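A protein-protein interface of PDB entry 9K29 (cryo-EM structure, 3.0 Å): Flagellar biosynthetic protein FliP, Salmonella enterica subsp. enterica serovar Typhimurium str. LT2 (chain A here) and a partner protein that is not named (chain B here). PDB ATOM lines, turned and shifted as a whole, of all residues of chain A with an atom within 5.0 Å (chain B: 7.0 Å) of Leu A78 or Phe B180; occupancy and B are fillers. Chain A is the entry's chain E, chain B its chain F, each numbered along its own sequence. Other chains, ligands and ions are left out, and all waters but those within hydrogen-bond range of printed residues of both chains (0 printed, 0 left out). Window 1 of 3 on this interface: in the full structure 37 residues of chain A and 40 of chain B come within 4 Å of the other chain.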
ATOM      1  N   LEU A  74     -20.122  16.445   1.547  1.00  0.00           N
ATOM      2  CA  LEU A  74     -19.850  16.155   0.142  1.00  0.00           C
ATOM      3  C   LEU A  74     -20.039  14.676  -0.170  1.00  0.00           C
ATOM      4  O   LEU A  74     -20.591  14.327  -1.222  1.00  0.00           O
ATOM      5  CB  LEU A  74     -18.435  16.599  -0.223  1.00  0.00           C
ATOM      6  CG  LEU A  74     -17.940  16.177  -1.606  1.00  0.00           C
ATOM      7  CD1 LEU A  74     -18.744  16.862  -2.697  1.00  0.00           C
ATOM      8  CD2 LEU A  74     -16.461  16.481  -1.760  1.00  0.00           C
ATOM      9  N   ARG A  75     -19.577  13.794   0.722  1.00  0.00           N
ATOM     10  CA  ARG A  75     -19.825  12.366   0.548  1.00  0.00           C
ATOM     11  C   ARG A  75     -21.316  12.079   0.455  1.00  0.00           C
ATOM     12  O   ARG A  75     -21.759  11.331  -0.424  1.00  0.00           O
ATOM     13  CB  ARG A  75     -19.224  11.574   1.708  1.00  0.00           C
ATOM     14  CG  ARG A  75     -17.721  11.603   1.795  1.00  0.00           C
ATOM     15  CD  ARG A  75     -17.274  11.205   3.191  1.00  0.00           C
ATOM     16  NE  ARG A  75     -17.468   9.789   3.473  1.00  0.00           N
ATOM     17  CZ  ARG A  75     -17.382   9.257   4.684  1.00  0.00           C
ATOM     18  NH1 ARG A  75     -17.106   9.996   5.746  1.00  0.00           N
ATOM     19  NH2 ARG A  75     -17.575   7.950   4.834  1.00  0.00           N
ATOM     20  N   ASN A  76     -22.103  12.663   1.360  1.00  0.00           N
ATOM     21  CA  ASN A  76     -23.550  12.484   1.304  1.00  0.00           C
ATOM     22  C   ASN A  76     -24.148  13.094   0.041  1.00  0.00           C
ATOM     23  O   ASN A  76     -25.110  12.551  -0.514  1.00  0.00           O
ATOM     24  CB  ASN A  76     -24.204  13.079   2.551  1.00  0.00           C
ATOM     25  CG  ASN A  76     -24.092  12.167   3.756  1.00  0.00           C
ATOM     26  OD1 ASN A  76     -25.051  11.493   4.127  1.00  0.00           O
ATOM     27  ND2 ASN A  76     -22.914  12.137   4.368  1.00  0.00           N
ATOM     28  N   ALA A  77     -23.598  14.218  -0.424  1.00  0.00           N
ATOM     29  CA  ALA A  77     -24.110  14.875  -1.621  1.00  0.00           C
ATOM     30  C   ALA A  77     -23.878  14.030  -2.862  1.00  0.00           C
ATOM     31  O   ALA A  77     -24.716  14.006  -3.769  1.00  0.00           O
ATOM     32  CB  ALA A  77     -23.455  16.245  -1.783  1.00  0.00           C
ATOM     33  N   LEU A  78     -22.746  13.334  -2.923  1.00  0.00           N
ATOM     34  CA  LEU A  78     -22.480  12.484  -4.074  1.00  0.00           C
ATOM     35  C   LEU A  78     -23.384  11.261  -4.129  1.00  0.00           C
ATOM     36  O   LEU A  78     -23.248  10.465  -5.062  1.00  0.00           O
ATOM     37  CB  LEU A  78     -21.014  12.049  -4.079  1.00  0.00           C
ATOM     38  CG  LEU A  78     -20.021  13.031  -4.700  1.00  0.00           C
ATOM     39  CD1 LEU A  78     -18.597  12.522  -4.550  1.00  0.00           C
ATOM     40  CD2 LEU A  78     -20.357  13.273  -6.161  1.00  0.00           C
ATOM     41  N   GLY A  79     -24.292  11.089  -3.169  1.00  0.00           N
ATOM     42  CA  GLY A  79     -25.180   9.942  -3.171  1.00  0.00           C
ATOM     43  C   GLY A  79     -24.483   8.622  -2.963  1.00  0.00           C
ATOM     44  O   GLY A  79     -25.084   7.566  -3.176  1.00  0.00           O
ATOM     45  N   THR A  80     -23.221   8.654  -2.545  1.00  0.00           N
ATOM     46  CA  THR A  80     -22.404   7.453  -2.383  1.00  0.00           C
ATOM     47  C   THR A  80     -21.713   7.482  -1.025  1.00  0.00           C
ATOM     48  O   THR A  80     -20.528   7.817  -0.907  1.00  0.00           O
ATOM     49  CB  THR A  80     -21.418   7.315  -3.550  1.00  0.00           C
ATOM     50  OG1 THR A  80     -20.657   6.105  -3.424  1.00  0.00           O
ATOM     51  CG2 THR A  80     -20.527   8.549  -3.716  1.00  0.00           C
ATOM     52  N   PRO A  84     -15.084   7.469  -0.612  1.00  0.00           N
ATOM     53  CA  PRO A  84     -13.680   7.498  -0.218  1.00  0.00           C
ATOM     54  C   PRO A  84     -13.537   7.115   1.243  1.00  0.00           C
ATOM     55  O   PRO A  84     -14.356   7.519   2.082  1.00  0.00           O
ATOM     56  CB  PRO A  84     -13.275   8.957  -0.465  1.00  0.00           C
ATOM     57  CG  PRO A  84     -14.524   9.725  -0.254  1.00  0.00           C
ATOM     58  CD  PRO A  84     -15.699   8.805  -0.484  1.00  0.00           C
ATOM     59  N   PHE A 193     -25.962  18.930  -6.763  1.00  0.00           N
ATOM     60  CA  PHE A 193     -26.284  17.507  -6.813  1.00  0.00           C
ATOM     61  C   PHE A 193     -27.770  17.260  -6.594  1.00  0.00           C
ATOM     62  O   PHE A 193     -28.338  16.338  -7.192  1.00  0.00           O
ATOM     63  CB  PHE A 193     -25.452  16.746  -5.784  1.00  0.00           C
ATOM     64  CG  PHE A 193     -23.975  16.806  -6.042  1.00  0.00           C
ATOM     65  CD1 PHE A 193     -23.458  16.398  -7.259  1.00  0.00           C
ATOM     66  CD2 PHE A 193     -23.106  17.279  -5.077  1.00  0.00           C
ATOM     67  CE1 PHE A 193     -22.101  16.453  -7.503  1.00  0.00           C
ATOM     68  CE2 PHE A 193     -21.749  17.336  -5.315  1.00  0.00           C
ATOM     69  CZ  PHE A 193     -21.245  16.923  -6.530  1.00  0.00           C
ATOM     70  N   LEU A 219     -26.227   8.590 -10.043  1.00  0.00           N
ATOM     71  CA  LEU A 219     -24.896   8.537  -9.441  1.00  0.00           C
ATOM     72  C   LEU A 219     -23.769   8.734 -10.450  1.00  0.00           C
ATOM     73  O   LEU A 219     -22.900   9.595 -10.210  1.00  0.00           O
ATOM     74  CB  LEU A 219     -24.742   7.218  -8.674  1.00  0.00           C
ATOM     75  CG  LEU A 219     -23.423   6.974  -7.947  1.00  0.00           C
ATOM     76  CD1 LEU A 219     -23.029   8.188  -7.139  1.00  0.00           C
ATOM     77  CD2 LEU A 219     -23.530   5.749  -7.064  1.00  0.00           C
ATOM     78  N   LYS A 222     -23.735  12.339 -11.519  1.00  0.00           N
ATOM     79  CA  LYS A 222     -23.214  13.203 -10.465  1.00  0.00           C
ATOM     80  C   LYS A 222     -21.693  13.151 -10.414  1.00  0.00           C
ATOM     81  O   LYS A 222     -21.036  14.194 -10.328  1.00  0.00           O
ATOM     82  CB  LYS A 222     -23.813  12.813  -9.114  1.00  0.00           C
ATOM     83  CG  LYS A 222     -25.278  13.181  -8.963  1.00  0.00           C
ATOM     84  CD  LYS A 222     -25.763  12.978  -7.538  1.00  0.00           C
ATOM     85  CE  LYS A 222     -25.940  11.506  -7.220  1.00  0.00           C
ATOM     86  NZ  LYS A 222     -26.550  11.304  -5.878  1.00  0.00           N
ATOM     87  N   LEU A 223     -21.112  11.950 -10.486  1.00  0.00           N
ATOM     88  CA  LEU A 223     -19.654  11.858 -10.452  1.00  0.00           C
ATOM     89  C   LEU A 223     -19.022  12.517 -11.673  1.00  0.00           C
ATOM     90  O   LEU A 223     -18.029  13.247 -11.548  1.00  0.00           O
ATOM     91  CB  LEU A 223     -19.204  10.402 -10.344  1.00  0.00           C
ATOM     92  CG  LEU A 223     -17.686  10.263 -10.187  1.00  0.00           C
ATOM     93  CD1 LEU A 223     -17.196  11.072  -8.994  1.00  0.00           C
ATOM     94  CD2 LEU A 223     -17.249   8.813 -10.066  1.00  0.00           C
ATOM     95  N   PHE A 226     -19.249  16.254 -11.327  1.00  0.00           N
ATOM     96  CA  PHE A 226     -18.330  16.719 -10.296  1.00  0.00           C
ATOM     97  C   PHE A 226     -16.892  16.738 -10.795  1.00  0.00           C
ATOM     98  O   PHE A 226     -16.119  17.627 -10.423  1.00  0.00           O
ATOM     99  CB  PHE A 226     -18.450  15.841  -9.053  1.00  0.00           C
ATOM    100  CG  PHE A 226     -17.491  16.206  -7.958  1.00  0.00           C
ATOM    101  CD1 PHE A 226     -17.621  17.403  -7.275  1.00  0.00           C
ATOM    102  CD2 PHE A 226     -16.460  15.352  -7.609  1.00  0.00           C
ATOM    103  CE1 PHE A 226     -16.741  17.740  -6.267  1.00  0.00           C
ATOM    104  CE2 PHE A 226     -15.577  15.684  -6.603  1.00  0.00           C
ATOM    105  CZ  PHE A 226     -15.718  16.880  -5.931  1.00  0.00           C
ATOM    106  N   VAL A 227     -16.514  15.772 -11.628  1.00  0.00           N
ATOM    107  CA  VAL A 227     -15.149  15.717 -12.141  1.00  0.00           C
ATOM    108  C   VAL A 227     -14.935  16.699 -13.290  1.00  0.00           C
ATOM    109  O   VAL A 227     -13.895  17.359 -13.358  1.00  0.00           O
ATOM    110  CB  VAL A 227     -14.805  14.273 -12.558  1.00  0.00           C
ATOM    111  CG1 VAL A 227     -13.464  14.227 -13.269  1.00  0.00           C
ATOM    112  CG2 VAL A 227     -14.787  13.374 -11.339  1.00  0.00           C
ATOM    113  N   TRP A 232     -13.271  19.370  -7.121  1.00  0.00           N
ATOM    114  CA  TRP A 232     -12.411  19.244  -5.947  1.00  0.00           C
ATOM    115  C   TRP A 232     -11.465  20.433  -5.826  1.00  0.00           C
ATOM    116  O   TRP A 232     -11.235  20.947  -4.724  1.00  0.00           O
ATOM    117  CB  TRP A 232     -11.630  17.934  -6.013  1.00  0.00           C
ATOM    118  CG  TRP A 232     -10.915  17.585  -4.746  1.00  0.00           C
ATOM    119  CD1 TRP A 232      -9.607  17.824  -4.450  1.00  0.00           C
ATOM    120  CD2 TRP A 232     -11.471  16.923  -3.605  1.00  0.00           C
ATOM    121  NE1 TRP A 232      -9.312  17.350  -3.196  1.00  0.00           N
ATOM    122  CE2 TRP A 232     -10.440  16.790  -2.656  1.00  0.00           C
ATOM    123  CE3 TRP A 232     -12.741  16.431  -3.292  1.00  0.00           C
ATOM    124  CZ2 TRP A 232     -10.640  16.189  -1.415  1.00  0.00           C
ATOM    125  CZ3 TRP A 232     -12.936  15.831  -2.062  1.00  0.00           C
ATOM    126  CH2 TRP A 232     -11.892  15.718  -1.138  1.00  0.00           C
ATOM    127  N   ALA B  93      -7.368   4.797  -2.636  1.00  0.00           N
ATOM    128  CA  ALA B  93      -8.657   5.459  -2.493  1.00  0.00           C
ATOM    129  C   ALA B  93      -9.370   5.558  -3.835  1.00  0.00           C
ATOM    130  O   ALA B  93     -10.584   5.351  -3.919  1.00  0.00           O
ATOM    131  CB  ALA B  93      -8.472   6.845  -1.876  1.00  0.00           C
ATOM    132  N   ALA B  94      -8.622   5.855  -4.900  1.00  0.00           N
ATOM    133  CA  ALA B  94      -9.217   5.971  -6.228  1.00  0.00           C
ATOM    134  C   ALA B  94      -9.745   4.629  -6.716  1.00  0.00           C
ATOM    135  O   ALA B  94     -10.853   4.547  -7.263  1.00  0.00           O
ATOM    136  CB  ALA B  94      -8.192   6.537  -7.210  1.00  0.00           C
ATOM    137  N   THR B  97     -12.844   3.797  -4.799  1.00  0.00           N
ATOM    138  CA  THR B  97     -13.964   4.595  -5.283  1.00  0.00           C
ATOM    139  C   THR B  97     -14.515   4.033  -6.586  1.00  0.00           C
ATOM    140  O   THR B  97     -15.734   3.923  -6.756  1.00  0.00           O
ATOM    141  CB  THR B  97     -13.528   6.047  -5.474  1.00  0.00           C
ATOM    142  OG1 THR B  97     -12.794   6.483  -4.323  1.00  0.00           O
ATOM    143  CG2 THR B  97     -14.737   6.945  -5.670  1.00  0.00           C
ATOM    144  N   PHE B 101     -18.270   2.522  -6.915  1.00  0.00           N
ATOM    145  CA  PHE B 101     -19.195   3.079  -7.897  1.00  0.00           C
ATOM    146  C   PHE B 101     -19.683   2.019  -8.873  1.00  0.00           C
ATOM    147  O   PHE B 101     -20.854   2.042  -9.270  1.00  0.00           O
ATOM    148  CB  PHE B 101     -18.545   4.234  -8.655  1.00  0.00           C
ATOM    149  CG  PHE B 101     -18.726   5.567  -7.994  1.00  0.00           C
ATOM    150  CD1 PHE B 101     -18.117   5.848  -6.786  1.00  0.00           C
ATOM    151  CD2 PHE B 101     -19.527   6.533  -8.576  1.00  0.00           C
ATOM    152  CE1 PHE B 101     -18.288   7.075  -6.178  1.00  0.00           C
ATOM    153  CE2 PHE B 101     -19.704   7.757  -7.973  1.00  0.00           C
ATOM    154  CZ  PHE B 101     -19.082   8.031  -6.776  1.00  0.00           C
ATOM    155  N   LEU B 104     -22.294  -0.057  -6.847  1.00  0.00           N
ATOM    156  CA  LEU B 104     -23.569   0.615  -6.616  1.00  0.00           C
ATOM    157  C   LEU B 104     -24.446   0.580  -7.860  1.00  0.00           C
ATOM    158  O   LEU B 104     -25.666   0.407  -7.763  1.00  0.00           O
ATOM    159  CB  LEU B 104     -23.333   2.052  -6.156  1.00  0.00           C
ATOM    160  CG  LEU B 104     -22.700   2.178  -4.769  1.00  0.00           C
ATOM    161  CD1 LEU B 104     -22.387   3.623  -4.434  1.00  0.00           C
ATOM    162  CD2 LEU B 104     -23.600   1.572  -3.714  1.00  0.00           C
ATOM    163  N   PHE B 113     -28.415   3.666  -0.770  1.00  0.00           N
ATOM    164  CA  PHE B 113     -29.217   4.616  -1.533  1.00  0.00           C
ATOM    165  C   PHE B 113     -30.469   5.028  -0.768  1.00  0.00           C
ATOM    166  O   PHE B 113     -30.836   6.208  -0.742  1.00  0.00           O
ATOM    167  CB  PHE B 113     -29.595   4.012  -2.886  1.00  0.00           C
ATOM    168  CG  PHE B 113     -28.514   4.116  -3.918  1.00  0.00           C
ATOM    169  CD1 PHE B 113     -27.760   5.270  -4.033  1.00  0.00           C
ATOM    170  CD2 PHE B 113     -28.254   3.062  -4.775  1.00  0.00           C
ATOM    171  CE1 PHE B 113     -26.765   5.370  -4.984  1.00  0.00           C
ATOM    172  CE2 PHE B 113     -27.260   3.155  -5.727  1.00  0.00           C
ATOM    173  CZ  PHE B 113     -26.515   4.311  -5.832  1.00  0.00           C
ATOM    174  N   GLY B 176      -5.743  15.963  -4.212  1.00  0.00           N
ATOM    175  CA  GLY B 176      -6.736  15.000  -3.777  1.00  0.00           C
ATOM    176  C   GLY B 176      -7.836  14.761  -4.790  1.00  0.00           C
ATOM    177  O   GLY B 176      -8.586  13.791  -4.679  1.00  0.00           O
ATOM    178  N   GLY B 177      -7.957  15.649  -5.775  1.00  0.00           N
ATOM    179  CA  GLY B 177      -8.932  15.468  -6.832  1.00  0.00           C
ATOM    180  C   GLY B 177      -8.673  14.294  -7.746  1.00  0.00           C
ATOM    181  O   GLY B 177      -9.545  13.950  -8.548  1.00  0.00           O
ATOM    182  N   LEU B 178      -7.496  13.670  -7.651  1.00  0.00           N
ATOM    183  CA  LEU B 178      -7.185  12.530  -8.505  1.00  0.00           C
ATOM    184  C   LEU B 178      -8.050  11.320  -8.178  1.00  0.00           C
ATOM    185  O   LEU B 178      -8.221  10.436  -9.025  1.00  0.00           O
ATOM    186  CB  LEU B 178      -5.705  12.170  -8.378  1.00  0.00           C
ATOM    187  CG  LEU B 178      -4.725  13.104  -9.086  1.00  0.00           C
ATOM    188  CD1 LEU B 178      -3.290  12.718  -8.766  1.00  0.00           C
ATOM    189  CD2 LEU B 178      -4.965  13.097 -10.586  1.00  0.00           C
ATOM    190  N   ILE B 179      -8.602  11.263  -6.960  1.00  0.00           N
ATOM    191  CA  ILE B 179      -9.430  10.124  -6.558  1.00  0.00           C
ATOM    192  C   ILE B 179     -10.575   9.926  -7.542  1.00  0.00           C
ATOM    193  O   ILE B 179     -10.692   8.879  -8.187  1.00  0.00           O
ATOM    194  CB  ILE B 179      -9.963  10.317  -5.128  1.00  0.00           C
ATOM    195  CG1 ILE B 179      -8.857  10.799  -4.192  1.00  0.00           C
ATOM    196  CG2 ILE B 179     -10.574   9.026  -4.610  1.00  0.00           C
ATOM    197  CD1 ILE B 179      -7.756   9.810  -4.009  1.00  0.00           C
ATOM    198  N   PHE B 180     -11.434  10.938  -7.672  1.00  0.00           N
ATOM    199  CA  PHE B 180     -12.629  10.801  -8.498  1.00  0.00           C
ATOM    200  C   PHE B 180     -12.281  10.711  -9.979  1.00  0.00           C
ATOM    201  O   PHE B 180     -12.932   9.975 -10.730  1.00  0.00           O
ATOM    202  CB  PHE B 180     -13.574  11.970  -8.230  1.00  0.00           C
ATOM    203  CG  PHE B 180     -13.777  12.256  -6.773  1.00  0.00           C
ATOM    204  CD1 PHE B 180     -14.656  11.497  -6.020  1.00  0.00           C
ATOM    205  CD2 PHE B 180     -13.077  13.273  -6.150  1.00  0.00           C
ATOM    206  CE1 PHE B 180     -14.842  11.755  -4.677  1.00  0.00           C
ATOM    207  CE2 PHE B 180     -13.257  13.533  -4.808  1.00  0.00           C
ATOM    208  CZ  PHE B 180     -14.141  12.775  -4.071  1.00  0.00           C
ATOM    209  N   LEU B 181     -11.264  11.456 -10.416  1.00  0.00           N
ATOM    210  CA  LEU B 181     -10.859  11.403 -11.818  1.00  0.00           C
ATOM    211  C   LEU B 181     -10.414  10.000 -12.207  1.00  0.00           C
ATOM    212  O   LEU B 181     -10.863   9.448 -13.220  1.00  0.00           O
ATOM    213  CB  LEU B 181      -9.742  12.416 -12.074  1.00  0.00           C
ATOM    214  CG  LEU B 181      -9.056  12.348 -13.437  1.00  0.00           C
ATOM    215  CD1 LEU B 181     -10.048  12.637 -14.548  1.00  0.00           C
ATOM    216  CD2 LEU B 181      -7.887  13.317 -13.492  1.00  0.00           C
ATOM    217  N   ASN B 182      -9.541   9.395 -11.399  1.00  0.00           N
ATOM    218  CA  ASN B 182      -9.086   8.043 -11.695  1.00  0.00           C
ATOM    219  C   ASN B 182     -10.189   7.019 -11.471  1.00  0.00           C
ATOM    220  O   ASN B 182     -10.215   5.985 -12.147  1.00  0.00           O
ATOM    221  CB  ASN B 182      -7.857   7.712 -10.853  1.00  0.00           C
ATOM    222  CG  ASN B 182      -6.667   8.580 -11.205  1.00  0.00           C
ATOM    223  OD1 ASN B 182      -6.033   9.173 -10.333  1.00  0.00           O
ATOM    224  ND2 ASN B 182      -6.356   8.661 -12.494  1.00  0.00           N
ATOM    225  N   GLY B 183     -11.112   7.288 -10.545  1.00  0.00           N
ATOM    226  CA  GLY B 183     -12.251   6.403 -10.376  1.00  0.00           C
ATOM    227  C   GLY B 183     -13.126   6.349 -11.611  1.00  0.00           C
ATOM    228  O   GLY B 183     -13.574   5.275 -12.019  1.00  0.00           O
ATOM    229  N   LEU B 184     -13.388   7.507 -12.221  1.00  0.00           N
ATOM    230  CA  LEU B 184     -14.087   7.507 -13.501  1.00  0.00           C
ATOM    231  C   LEU B 184     -13.269   6.814 -14.580  1.00  0.00           C
ATOM    232  O   LEU B 184     -13.756   5.883 -15.230  1.00  0.00           O
ATOM    233  CB  LEU B 184     -14.428   8.931 -13.939  1.00  0.00           C
ATOM    234  CG  LEU B 184     -15.651   9.584 -13.308  1.00  0.00           C
ATOM    235  CD1 LEU B 184     -15.792  11.001 -13.814  1.00  0.00           C
ATOM    236  CD2 LEU B 184     -16.890   8.775 -13.644  1.00  0.00           C
ATOM    237  N   MET B 185     -12.011   7.229 -14.764  1.00  0.00           N
ATOM    238  CA  MET B 185     -11.214   6.703 -15.869  1.00  0.00           C
ATOM    239  C   MET B 185     -11.066   5.189 -15.782  1.00  0.00           C
ATOM    240  O   MET B 185     -10.937   4.511 -16.808  1.00  0.00           O
ATOM    241  CB  MET B 185      -9.845   7.379 -15.902  1.00  0.00           C
ATOM    242  CG  MET B 185      -9.902   8.865 -16.207  1.00  0.00           C
ATOM    243  SD  MET B 185     -10.553   9.193 -17.857  1.00  0.00           S
ATOM    244  CE  MET B 185     -10.715  10.976 -17.815  1.00  0.00           C
ATOM    245  N   LEU B 186     -11.081   4.640 -14.567  1.00  0.00           N
ATOM    246  CA  LEU B 186     -10.997   3.192 -14.418  1.00  0.00           C
ATOM    247  C   LEU B 186     -12.344   2.523 -14.669  1.00  0.00           C
ATOM    248  O   LEU B 186     -12.397   1.375 -15.124  1.00  0.00           O
ATOM    249  CB  LEU B 186     -10.470   2.842 -13.028  1.00  0.00           C
ATOM    250  CG  LEU B 186     -10.227   1.363 -12.735  1.00  0.00           C
ATOM    251  CD1 LEU B 186      -9.249   0.777 -13.735  1.00  0.00           C
ATOM    252  CD2 LEU B 186      -9.700   1.198 -11.323  1.00  0.00           C
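NE1 of Trp A232 sits close to N of Gly B177, at 3.4 Å.
Phe B101 touches Thr A80.
OG1 of Thr A80 touches CD1 of Leu B104, at 3.2 Å.
Leu B104 touches Leu A219 (CD1 to CD2, 3.6 Å).
Leu A219 touches Phe B113 (CD2 to CZ, 3.5 Å).
Leu A223 touches Phe B101 (CD2 to CE2, 3.4 Å).
CD1 of Leu A223 touches CB of Phe B180, at 3.8 Å.
CD2 of Phe B180 touches CE2 of Phe A226, at 3.5 Å.
Val A227 touches Phe B180.
Val A227 touches Leu B181.
Phe B180 touches Trp A232.
Leu A78 touches one residue of chain B.
Of the printed residues of chain B, Thr A80 touches Phe B101 (3.4 Å) and Leu B104 (3.2 Å).
Of the printed residues of chain B, Leu A223 touches Phe B101 (3.4 Å), Phe B180 (3.8 Å) and Leu B184 (3.6 Å).
Printed residues of chain B within 4 Å of Trp A232: Gly B176 (3.4 Å), Gly B177 (3.0 Å) and Phe B180 (3.3 Å).
Of the printed residues of chain A, Phe B101 touches Thr A80 (3.4 Å), Leu A219 (3.5 Å) and Leu A223 (3.4 Å).
Of chain A, only Leu A78 (3.8 Å), Leu A223 (3.8 Å), Phe A226 (3.5 Å), Val A227 (3.6 Å) and Trp A232 (3.3 Å) come within 4 Å of Phe B180.
Hydrophobic or aromatic side chains of chain A within 4 Å of the printed part of chain B: Leu A78, Leu A219, Leu A223, Phe A226, Val A227 and Trp A232.
Of the 17 printed residues of chain B, 8 touch a printed residue of chain A.
Printed residues of chain B that touch a printed residue of chain A: Phe B101, Leu B104, Phe B113, Gly B176, Gly B177, Phe B180, Leu B181 and Leu B184.
Hydrophobic or aromatic side chains of chain B that line the printed part of chain A: Phe B101, Leu B104, Phe B113, Phe B180, Leu B181 and Leu B184.
Among the printed residues, 17 pairs touch across the chains.
Among the printed residues, no Asp or Glu carboxylate lies within 4 Å of a Lys or Arg side-chain nitrogen of the other chain.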
